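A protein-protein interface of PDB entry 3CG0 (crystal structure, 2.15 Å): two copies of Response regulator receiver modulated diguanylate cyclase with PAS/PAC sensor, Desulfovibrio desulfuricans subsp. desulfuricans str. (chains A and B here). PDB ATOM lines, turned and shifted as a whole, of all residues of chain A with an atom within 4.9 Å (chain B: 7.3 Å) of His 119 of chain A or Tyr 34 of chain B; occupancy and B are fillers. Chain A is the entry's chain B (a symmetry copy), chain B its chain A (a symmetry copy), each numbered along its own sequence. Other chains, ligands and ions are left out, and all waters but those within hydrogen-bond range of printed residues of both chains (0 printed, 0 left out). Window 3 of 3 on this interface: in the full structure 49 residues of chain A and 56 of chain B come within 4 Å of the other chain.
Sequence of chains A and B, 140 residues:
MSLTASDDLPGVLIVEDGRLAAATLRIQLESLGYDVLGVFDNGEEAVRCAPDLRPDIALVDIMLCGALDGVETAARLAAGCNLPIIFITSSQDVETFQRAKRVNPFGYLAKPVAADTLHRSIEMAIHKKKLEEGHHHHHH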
ATOM      1  N   ALA A 115      35.364  13.521  24.395  1.00  0.00           N
ATOM      2  CA  ALA A 115      34.615  13.956  23.217  1.00  0.00           C
ATOM      3  C   ALA A 115      34.340  12.837  22.204  1.00  0.00           C
ATOM      4  O   ALA A 115      33.201  12.686  21.741  1.00  0.00           O
ATOM      5  CB  ALA A 115      35.352  15.107  22.530  1.00  0.00           C
ATOM      6  N   ASP A 116      35.371  12.063  21.877  1.00  0.00           N
ATOM      7  CA  ASP A 116      35.255  10.964  20.898  1.00  0.00           C
ATOM      8  C   ASP A 116      34.221   9.940  21.339  1.00  0.00           C
ATOM      9  O   ASP A 116      33.383   9.520  20.554  1.00  0.00           O
ATOM     10  CB  ASP A 116      36.611  10.268  20.675  1.00  0.00           C
ATOM     11  CG  ASP A 116      36.496   8.971  19.855  1.00  0.00           C
ATOM     12  OD1 ASP A 116      35.977   9.014  18.713  1.00  0.00           O
ATOM     13  OD2 ASP A 116      36.943   7.908  20.347  1.00  0.00           O
ATOM     14  N   THR A 117      34.307   9.544  22.604  1.00  0.00           N
ATOM     15  CA  THR A 117      33.438   8.542  23.204  1.00  0.00           C
ATOM     16  C   THR A 117      32.010   9.075  23.344  1.00  0.00           C
ATOM     17  O   THR A 117      31.042   8.324  23.194  1.00  0.00           O
ATOM     18  CB  THR A 117      33.982   8.158  24.573  1.00  0.00           C
ATOM     19  OG1 THR A 117      35.406   8.042  24.485  1.00  0.00           O
ATOM     20  CG2 THR A 117      33.381   6.833  25.074  1.00  0.00           C
ATOM     21  N   LEU A 118      31.901  10.370  23.635  1.00  0.00           N
ATOM     22  CA  LEU A 118      30.632  11.075  23.718  1.00  0.00           C
ATOM     23  C   LEU A 118      29.898  11.116  22.383  1.00  0.00           C
ATOM     24  O   LEU A 118      28.707  10.804  22.327  1.00  0.00           O
ATOM     25  CB  LEU A 118      30.858  12.505  24.227  1.00  0.00           C
ATOM     26  CG  LEU A 118      29.669  13.464  24.260  1.00  0.00           C
ATOM     27  CD1 LEU A 118      28.607  12.966  25.234  1.00  0.00           C
ATOM     28  CD2 LEU A 118      30.161  14.845  24.649  1.00  0.00           C
ATOM     29  N   HIS A 119      30.604  11.499  21.316  1.00  0.00           N
ATOM     30  CA  HIS A 119      30.027  11.522  19.976  1.00  0.00           C
ATOM     31  C   HIS A 119      29.617  10.131  19.507  1.00  0.00           C
ATOM     32  O   HIS A 119      28.541   9.972  18.937  1.00  0.00           O
ATOM     33  CB  HIS A 119      31.002  12.102  18.948  1.00  0.00           C
ATOM     34  CG  HIS A 119      30.656  11.740  17.532  1.00  0.00           C
ATOM     35  ND1 HIS A 119      29.588  12.300  16.861  1.00  0.00           N
ATOM     36  CD2 HIS A 119      31.208  10.844  16.678  1.00  0.00           C
ATOM     37  CE1 HIS A 119      29.505  11.773  15.652  1.00  0.00           C
ATOM     38  NE2 HIS A 119      30.477  10.888  15.515  1.00  0.00           N
ATOM     39  N   ARG A 120      30.502   9.155  19.709  1.00  0.00           N
ATOM     40  CA  ARG A 120      30.293   7.784  19.241  1.00  0.00           C
ATOM     41  C   ARG A 120      29.169   7.095  19.982  1.00  0.00           C
ATOM     42  O   ARG A 120      28.460   6.287  19.394  1.00  0.00           O
ATOM     43  CB  ARG A 120      31.560   6.931  19.383  1.00  0.00           C
ATOM     44  CG  ARG A 120      32.658   7.189  18.379  1.00  0.00           C
ATOM     45  CD  ARG A 120      32.196   7.128  16.939  1.00  0.00           C
ATOM     46  NE  ARG A 120      33.344   7.272  16.048  1.00  0.00           N
ATOM     47  CZ  ARG A 120      33.297   7.785  14.823  1.00  0.00           C
ATOM     48  NH1 ARG A 120      34.406   7.860  14.101  1.00  0.00           N
ATOM     49  NH2 ARG A 120      32.152   8.230  14.322  1.00  0.00           N
ATOM     50  N   SER A 121      29.032   7.392  21.275  1.00  0.00           N
ATOM     51  CA  SER A 121      27.912   6.879  22.069  1.00  0.00           C
ATOM     52  C   SER A 121      26.587   7.470  21.651  1.00  0.00           C
ATOM     53  O   SER A 121      25.613   6.731  21.473  1.00  0.00           O
ATOM     54  CB  SER A 121      28.149   7.083  23.555  1.00  0.00           C
ATOM     55  OG  SER A 121      29.146   6.160  23.966  1.00  0.00           O
ATOM     56  N   ILE A 122      26.557   8.790  21.457  1.00  0.00           N
ATOM     57  CA  ILE A 122      25.358   9.455  20.959  1.00  0.00           C
ATOM     58  C   ILE A 122      24.910   8.905  19.602  1.00  0.00           C
ATOM     59  O   ILE A 122      23.732   8.628  19.411  1.00  0.00           O
ATOM     60  CB  ILE A 122      25.529  10.973  20.905  1.00  0.00           C
ATOM     61  CG1 ILE A 122      25.579  11.538  22.325  1.00  0.00           C
ATOM     62  CG2 ILE A 122      24.398  11.617  20.112  1.00  0.00           C
ATOM     63  CD1 ILE A 122      25.516  13.031  22.363  1.00  0.00           C
ATOM     64  N   GLU A 123      25.851   8.715  18.679  1.00  0.00           N
ATOM     65  CA  GLU A 123      25.491   8.266  17.338  1.00  0.00           C
ATOM     66  C   GLU A 123      25.110   6.782  17.242  1.00  0.00           C
ATOM     67  O   GLU A 123      24.263   6.432  16.423  1.00  0.00           O
ATOM     68  CB  GLU A 123      26.555   8.655  16.296  1.00  0.00           C
ATOM     69  CG  GLU A 123      27.850   7.874  16.357  1.00  0.00           C
ATOM     70  CD  GLU A 123      28.431   7.598  14.978  1.00  0.00           C
ATOM     71  OE1 GLU A 123      28.445   8.525  14.143  1.00  0.00           O
ATOM     72  OE2 GLU A 123      28.877   6.453  14.728  1.00  0.00           O
ATOM     73  N   LEU B   9      21.133  19.254  12.675  1.00  0.00           N
ATOM     74  CA  LEU B   9      21.851  18.900  13.904  1.00  0.00           C
ATOM     75  C   LEU B   9      21.011  17.937  14.747  1.00  0.00           C
ATOM     76  O   LEU B   9      19.819  18.192  14.963  1.00  0.00           O
ATOM     77  CB  LEU B   9      22.189  20.150  14.738  1.00  0.00           C
ATOM     78  CG  LEU B   9      22.554  21.502  14.106  1.00  0.00           C
ATOM     79  CD1 LEU B   9      21.318  22.386  13.898  1.00  0.00           C
ATOM     80  CD2 LEU B   9      23.600  22.238  14.939  1.00  0.00           C
ATOM     81  N   PRO B  10      21.620  16.824  15.218  1.00  0.00           N
ATOM     82  CA  PRO B  10      20.931  15.980  16.195  1.00  0.00           C
ATOM     83  C   PRO B  10      20.806  16.752  17.511  1.00  0.00           C
ATOM     84  O   PRO B  10      21.754  17.424  17.936  1.00  0.00           O
ATOM     85  CB  PRO B  10      21.856  14.768  16.350  1.00  0.00           C
ATOM     86  CG  PRO B  10      22.830  14.860  15.237  1.00  0.00           C
ATOM     87  CD  PRO B  10      22.958  16.298  14.895  1.00  0.00           C
ATOM     88  N   GLY B  11      19.623  16.692  18.110  1.00  0.00           N
ATOM     89  CA  GLY B  11      19.305  17.509  19.268  1.00  0.00           C
ATOM     90  C   GLY B  11      19.453  16.765  20.574  1.00  0.00           C
ATOM     91  O   GLY B  11      18.844  15.711  20.772  1.00  0.00           O
ATOM     92  N   VAL B  12      20.267  17.319  21.467  1.00  0.00           N
ATOM     93  CA  VAL B  12      20.579  16.675  22.739  1.00  0.00           C
ATOM     94  C   VAL B  12      19.952  17.419  23.915  1.00  0.00           C
ATOM     95  O   VAL B  12      20.049  18.639  24.011  1.00  0.00           O
ATOM     96  CB  VAL B  12      22.111  16.544  22.957  1.00  0.00           C
ATOM     97  CG1 VAL B  12      22.424  15.789  24.260  1.00  0.00           C
ATOM     98  CG2 VAL B  12      22.749  15.831  21.784  1.00  0.00           C
ATOM     99  N   ARG B  26      28.286  21.034  27.281  1.00  0.00           N
ATOM    100  CA  ARG B  26      27.760  21.979  26.304  1.00  0.00           C
ATOM    101  C   ARG B  26      28.829  22.269  25.262  1.00  0.00           C
ATOM    102  O   ARG B  26      28.566  22.165  24.068  1.00  0.00           O
ATOM    103  CB  ARG B  26      27.322  23.280  26.976  1.00  0.00           C
ATOM    104  CG  ARG B  26      26.642  24.291  26.041  1.00  0.00           C
ATOM    105  CD  ARG B  26      25.645  25.177  26.825  1.00  0.00           C
ATOM    106  NE  ARG B  26      24.362  25.258  26.134  1.00  0.00           N
ATOM    107  CZ  ARG B  26      23.185  25.338  26.746  1.00  0.00           C
ATOM    108  NH1 ARG B  26      23.110  25.366  28.070  1.00  0.00           N
ATOM    109  NH2 ARG B  26      22.078  25.395  26.030  1.00  0.00           N
ATOM    110  N   GLN B  28      31.768  20.654  24.518  1.00  0.00           N
ATOM    111  CA  GLN B  28      32.051  19.444  23.756  1.00  0.00           C
ATOM    112  C   GLN B  28      31.028  19.180  22.653  1.00  0.00           C
ATOM    113  O   GLN B  28      31.397  18.975  21.491  1.00  0.00           O
ATOM    114  CB  GLN B  28      32.096  18.235  24.683  1.00  0.00           C
ATOM    115  CG  GLN B  28      33.386  18.064  25.423  1.00  0.00           C
ATOM    116  CD  GLN B  28      33.312  16.981  26.455  1.00  0.00           C
ATOM    117  OE1 GLN B  28      32.245  16.703  27.003  1.00  0.00           O
ATOM    118  NE2 GLN B  28      34.451  16.364  26.746  1.00  0.00           N
ATOM    119  N   LEU B  29      29.748  19.198  23.022  1.00  0.00           N
ATOM    120  CA  LEU B  29      28.668  18.872  22.095  1.00  0.00           C
ATOM    121  C   LEU B  29      28.487  19.917  20.999  1.00  0.00           C
ATOM    122  O   LEU B  29      28.340  19.574  19.817  1.00  0.00           O
ATOM    123  CB  LEU B  29      27.353  18.643  22.849  1.00  0.00           C
ATOM    124  CG  LEU B  29      27.244  17.358  23.675  1.00  0.00           C
ATOM    125  CD1 LEU B  29      26.052  17.432  24.597  1.00  0.00           C
ATOM    126  CD2 LEU B  29      27.157  16.147  22.793  1.00  0.00           C
ATOM    127  N   GLU B  30      28.529  21.189  21.381  1.00  0.00           N
ATOM    128  CA  GLU B  30      28.450  22.269  20.400  1.00  0.00           C
ATOM    129  C   GLU B  30      29.635  22.276  19.426  1.00  0.00           C
ATOM    130  O   GLU B  30      29.478  22.686  18.273  1.00  0.00           O
ATOM    131  CB  GLU B  30      28.306  23.623  21.082  1.00  0.00           C
ATOM    132  CG  GLU B  30      26.925  23.848  21.660  1.00  0.00           C
ATOM    133  CD  GLU B  30      26.782  25.175  22.353  1.00  0.00           C
ATOM    134  OE1 GLU B  30      27.817  25.859  22.575  1.00  0.00           O
ATOM    135  OE2 GLU B  30      25.625  25.528  22.680  1.00  0.00           O
ATOM    136  N   SER B  31      30.804  21.817  19.879  1.00  0.00           N
ATOM    137  CA  SER B  31      31.948  21.673  18.979  1.00  0.00           C
ATOM    138  C   SER B  31      31.732  20.529  17.999  1.00  0.00           C
ATOM    139  O   SER B  31      31.930  20.699  16.797  1.00  0.00           O
ATOM    140  CB  SER B  31      33.252  21.464  19.741  1.00  0.00           C
ATOM    141  OG  SER B  31      33.629  22.652  20.410  1.00  0.00           O
ATOM    142  N   LEU B  32      31.290  19.383  18.505  1.00  0.00           N
ATOM    143  CA  LEU B  32      31.168  18.177  17.676  1.00  0.00           C
ATOM    144  C   LEU B  32      30.073  18.261  16.606  1.00  0.00           C
ATOM    145  O   LEU B  32      29.993  17.392  15.732  1.00  0.00           O
ATOM    146  CB  LEU B  32      30.978  16.936  18.558  1.00  0.00           C
ATOM    147  CG  LEU B  32      32.135  16.555  19.486  1.00  0.00           C
ATOM    148  CD1 LEU B  32      31.626  15.702  20.631  1.00  0.00           C
ATOM    149  CD2 LEU B  32      33.278  15.864  18.754  1.00  0.00           C
ATOM    150  N   GLY B  33      29.245  19.303  16.681  1.00  0.00           N
ATOM    151  CA  GLY B  33      28.143  19.522  15.746  1.00  0.00           C
ATOM    152  C   GLY B  33      26.779  19.047  16.227  1.00  0.00           C
ATOM    153  O   GLY B  33      26.036  18.410  15.470  1.00  0.00           O
ATOM    154  N   TYR B  34      26.450  19.345  17.485  1.00  0.00           N
ATOM    155  CA  TYR B  34      25.158  18.968  18.058  1.00  0.00           C
ATOM    156  C   TYR B  34      24.376  20.187  18.485  1.00  0.00           C
ATOM    157  O   TYR B  34      24.962  21.222  18.810  1.00  0.00           O
ATOM    158  CB  TYR B  34      25.328  18.039  19.262  1.00  0.00           C
ATOM    159  CG  TYR B  34      25.734  16.620  18.903  1.00  0.00           C
ATOM    160  CD1 TYR B  34      24.807  15.728  18.382  1.00  0.00           C
ATOM    161  CD2 TYR B  34      27.035  16.178  19.100  1.00  0.00           C
ATOM    162  CE1 TYR B  34      25.168  14.438  18.056  1.00  0.00           C
ATOM    163  CE2 TYR B  34      27.413  14.882  18.779  1.00  0.00           C
ATOM    164  CZ  TYR B  34      26.467  14.017  18.251  1.00  0.00           C
ATOM    165  OH  TYR B  34      26.810  12.725  17.916  1.00  0.00           O
ATOM    166  N   ASP B  35      23.051  20.054  18.484  1.00  0.00           N
ATOM    167  CA  ASP B  35      22.165  21.091  18.988  1.00  0.00           C
ATOM    168  C   ASP B  35      21.859  20.790  20.450  1.00  0.00           C
ATOM    169  O   ASP B  35      21.125  19.853  20.759  1.00  0.00           O
ATOM    170  CB  ASP B  35      20.876  21.145  18.153  1.00  0.00           C
ATOM    171  CG  ASP B  35      20.081  22.439  18.348  1.00  0.00           C
ATOM    172  OD1 ASP B  35      20.258  23.141  19.368  1.00  0.00           O
ATOM    173  OD2 ASP B  35      19.244  22.748  17.468  1.00  0.00           O
ATOM    174  N   VAL B  36      22.431  21.575  21.356  1.00  0.00           N
ATOM    175  CA  VAL B  36      22.105  21.407  22.767  1.00  0.00           C
ATOM    176  C   VAL B  36      20.798  22.123  23.044  1.00  0.00           C
ATOM    177  O   VAL B  36      20.718  23.353  23.012  1.00  0.00           O
ATOM    178  CB  VAL B  36      23.248  21.816  23.741  1.00  0.00           C
ATOM    179  CG1 VAL B  36      22.820  21.604  25.194  1.00  0.00           C
ATOM    180  CG2 VAL B  36      24.485  20.980  23.473  1.00  0.00           C
ATOM    181  N   LEU B  37      19.777  21.313  23.309  1.00  0.00           N
ATOM    182  CA  LEU B  37      18.396  21.753  23.362  1.00  0.00           C
ATOM    183  C   LEU B  37      18.007  22.366  24.693  1.00  0.00           C
ATOM    184  O   LEU B  37      17.116  23.206  24.751  1.00  0.00           O
ATOM    185  CB  LEU B  37      17.459  20.585  23.003  1.00  0.00           C
ATOM    186  CG  LEU B  37      16.815  20.556  21.607  1.00  0.00           C
ATOM    187  CD1 LEU B  37      17.628  21.249  20.549  1.00  0.00           C
ATOM    188  CD2 LEU B  37      16.565  19.134  21.177  1.00  0.00           C
ATOM    189  N   ILE B  57      18.035  12.556  21.799  1.00  0.00           N
ATOM    190  CA  ILE B  57      18.749  11.813  22.843  1.00  0.00           C
ATOM    191  C   ILE B  57      18.775  12.603  24.171  1.00  0.00           C
ATOM    192  O   ILE B  57      18.805  13.841  24.181  1.00  0.00           O
ATOM    193  CB  ILE B  57      20.197  11.398  22.330  1.00  0.00           C
ATOM    194  CG1 ILE B  57      20.676  10.044  22.890  1.00  0.00           C
ATOM    195  CG2 ILE B  57      21.216  12.526  22.448  1.00  0.00           C
ATOM    196  CD1 ILE B  57      21.295  10.045  24.252  1.00  0.00           C
ATOM    197  N   ILE B  86      21.498   7.941  27.740  1.00  0.00           N
ATOM    198  CA  ILE B  86      22.832   7.625  28.224  1.00  0.00           C
ATOM    199  C   ILE B  86      22.962   8.261  29.605  1.00  0.00           C
ATOM    200  O   ILE B  86      22.734   9.464  29.772  1.00  0.00           O
ATOM    201  CB  ILE B  86      23.934   8.120  27.245  1.00  0.00           C
ATOM    202  CG1 ILE B  86      23.831   7.414  25.887  1.00  0.00           C
ATOM    203  CG2 ILE B  86      25.333   7.899  27.835  1.00  0.00           C
ATOM    204  CD1 ILE B  86      24.542   8.148  24.739  1.00  0.00           C
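The side-chain hydroxyl (OH) of Tyr 34 of chain B is in hydrogen-bond range of a ring nitrogen (ND1) of His 119 of chain A (3.0 Å).
No position is printed for both chains.
Among the printed residues, pairs that only touch across the chains: Ala 115 of chain A with Gln 28 of chain B (3.8 Å), Ala 115 of chain A with Leu 32 of chain B (3.6 Å), Leu 118 of chain A with Gln 28 of chain B (3.7 Å), Leu 118 of chain A with Leu 29 of chain B (3.8 Å), Ser 121 of chain A with Ile 86 of chain B (3.7 Å), Ile 122 of chain A with Val 12 of chain B (3.98 Å), Ile 122 of chain A with Leu 29 of chain B (3.5 Å), Ile 122 of chain A with Tyr 34 of chain B (3.4 Å) and Ile 122 of chain A with Ile 86 of chain B (3.9 Å).
Of the 9 printed residues of chain A, 5 touch a printed residue of chain B.
Hydrophobic or aromatic side chains of chain A that line the printed part of chain B: Leu 118, His 119 and Ile 122.
Printed residues of chain B that touch a printed residue of chain A: Val 12, Gln 28, Leu 29, Leu 32, Tyr 34 and Ile 86.
Among the printed residues, 10 pairs touch across the chains.
Of chain B, only Tyr 34 (3.0 Å) comes within 4 Å of His 119 of chain A.
Of the printed residues of chain B, Ser 121 of chain A touches Ile 86.
Of the printed residues of chain A, Gln 28 of chain B touches Ala 115 and Leu 118.
Of the printed residues of chain A, Leu 29 of chain B touches Leu 118 and Ile 122.
Ser 31 of chain B touches none of the printed residues of chain A.
Printed residues of chain A within 4 Å of Leu 32 of chain B: Ala 115 (3.6 Å).
Gly 33 of chain B touches none of the printed residues of chain A.
Of the printed residues of chain A, Tyr 34 of chain B touches His 119 (3.0 Å) and Ile 122 (3.4 Å).
The nearest residue of chain B that does not touch His 119 of chain A is Leu 32 of chain B (4.02 Å).
The nearest residue of chain A that does not touch Tyr 34 of chain B is Glu 123 of chain A (4.2 Å).
O of Asp 35 of chain B lies within hydrogen-bond range of N of Val 12 of chain B.
The backbone carbonyl oxygen of Val 12 of chain B is in hydrogen-bond range of the backbone NH of Leu 37 of chain B (2.8 Å).
O of Leu 29 of chain B sits at hydrogen-bond distance from N of Tyr 34 of chain B (3.0 Å).
OG of Ser 121 of chain A sits at hydrogen-bond distance from O of Thr 117 of chain A, 3.0 Å away.
A ring nitrogen (NE2) of His 119 of chain A sits at hydrogen-bond distance from the guanidinium group (NH2) of Arg 120 of chain A (3.4 Å).
A ring nitrogen (NE2) of His 119 of chain A lies within hydrogen-bond range of the side-chain carboxylate (OE1) of Glu 123 of chain A.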
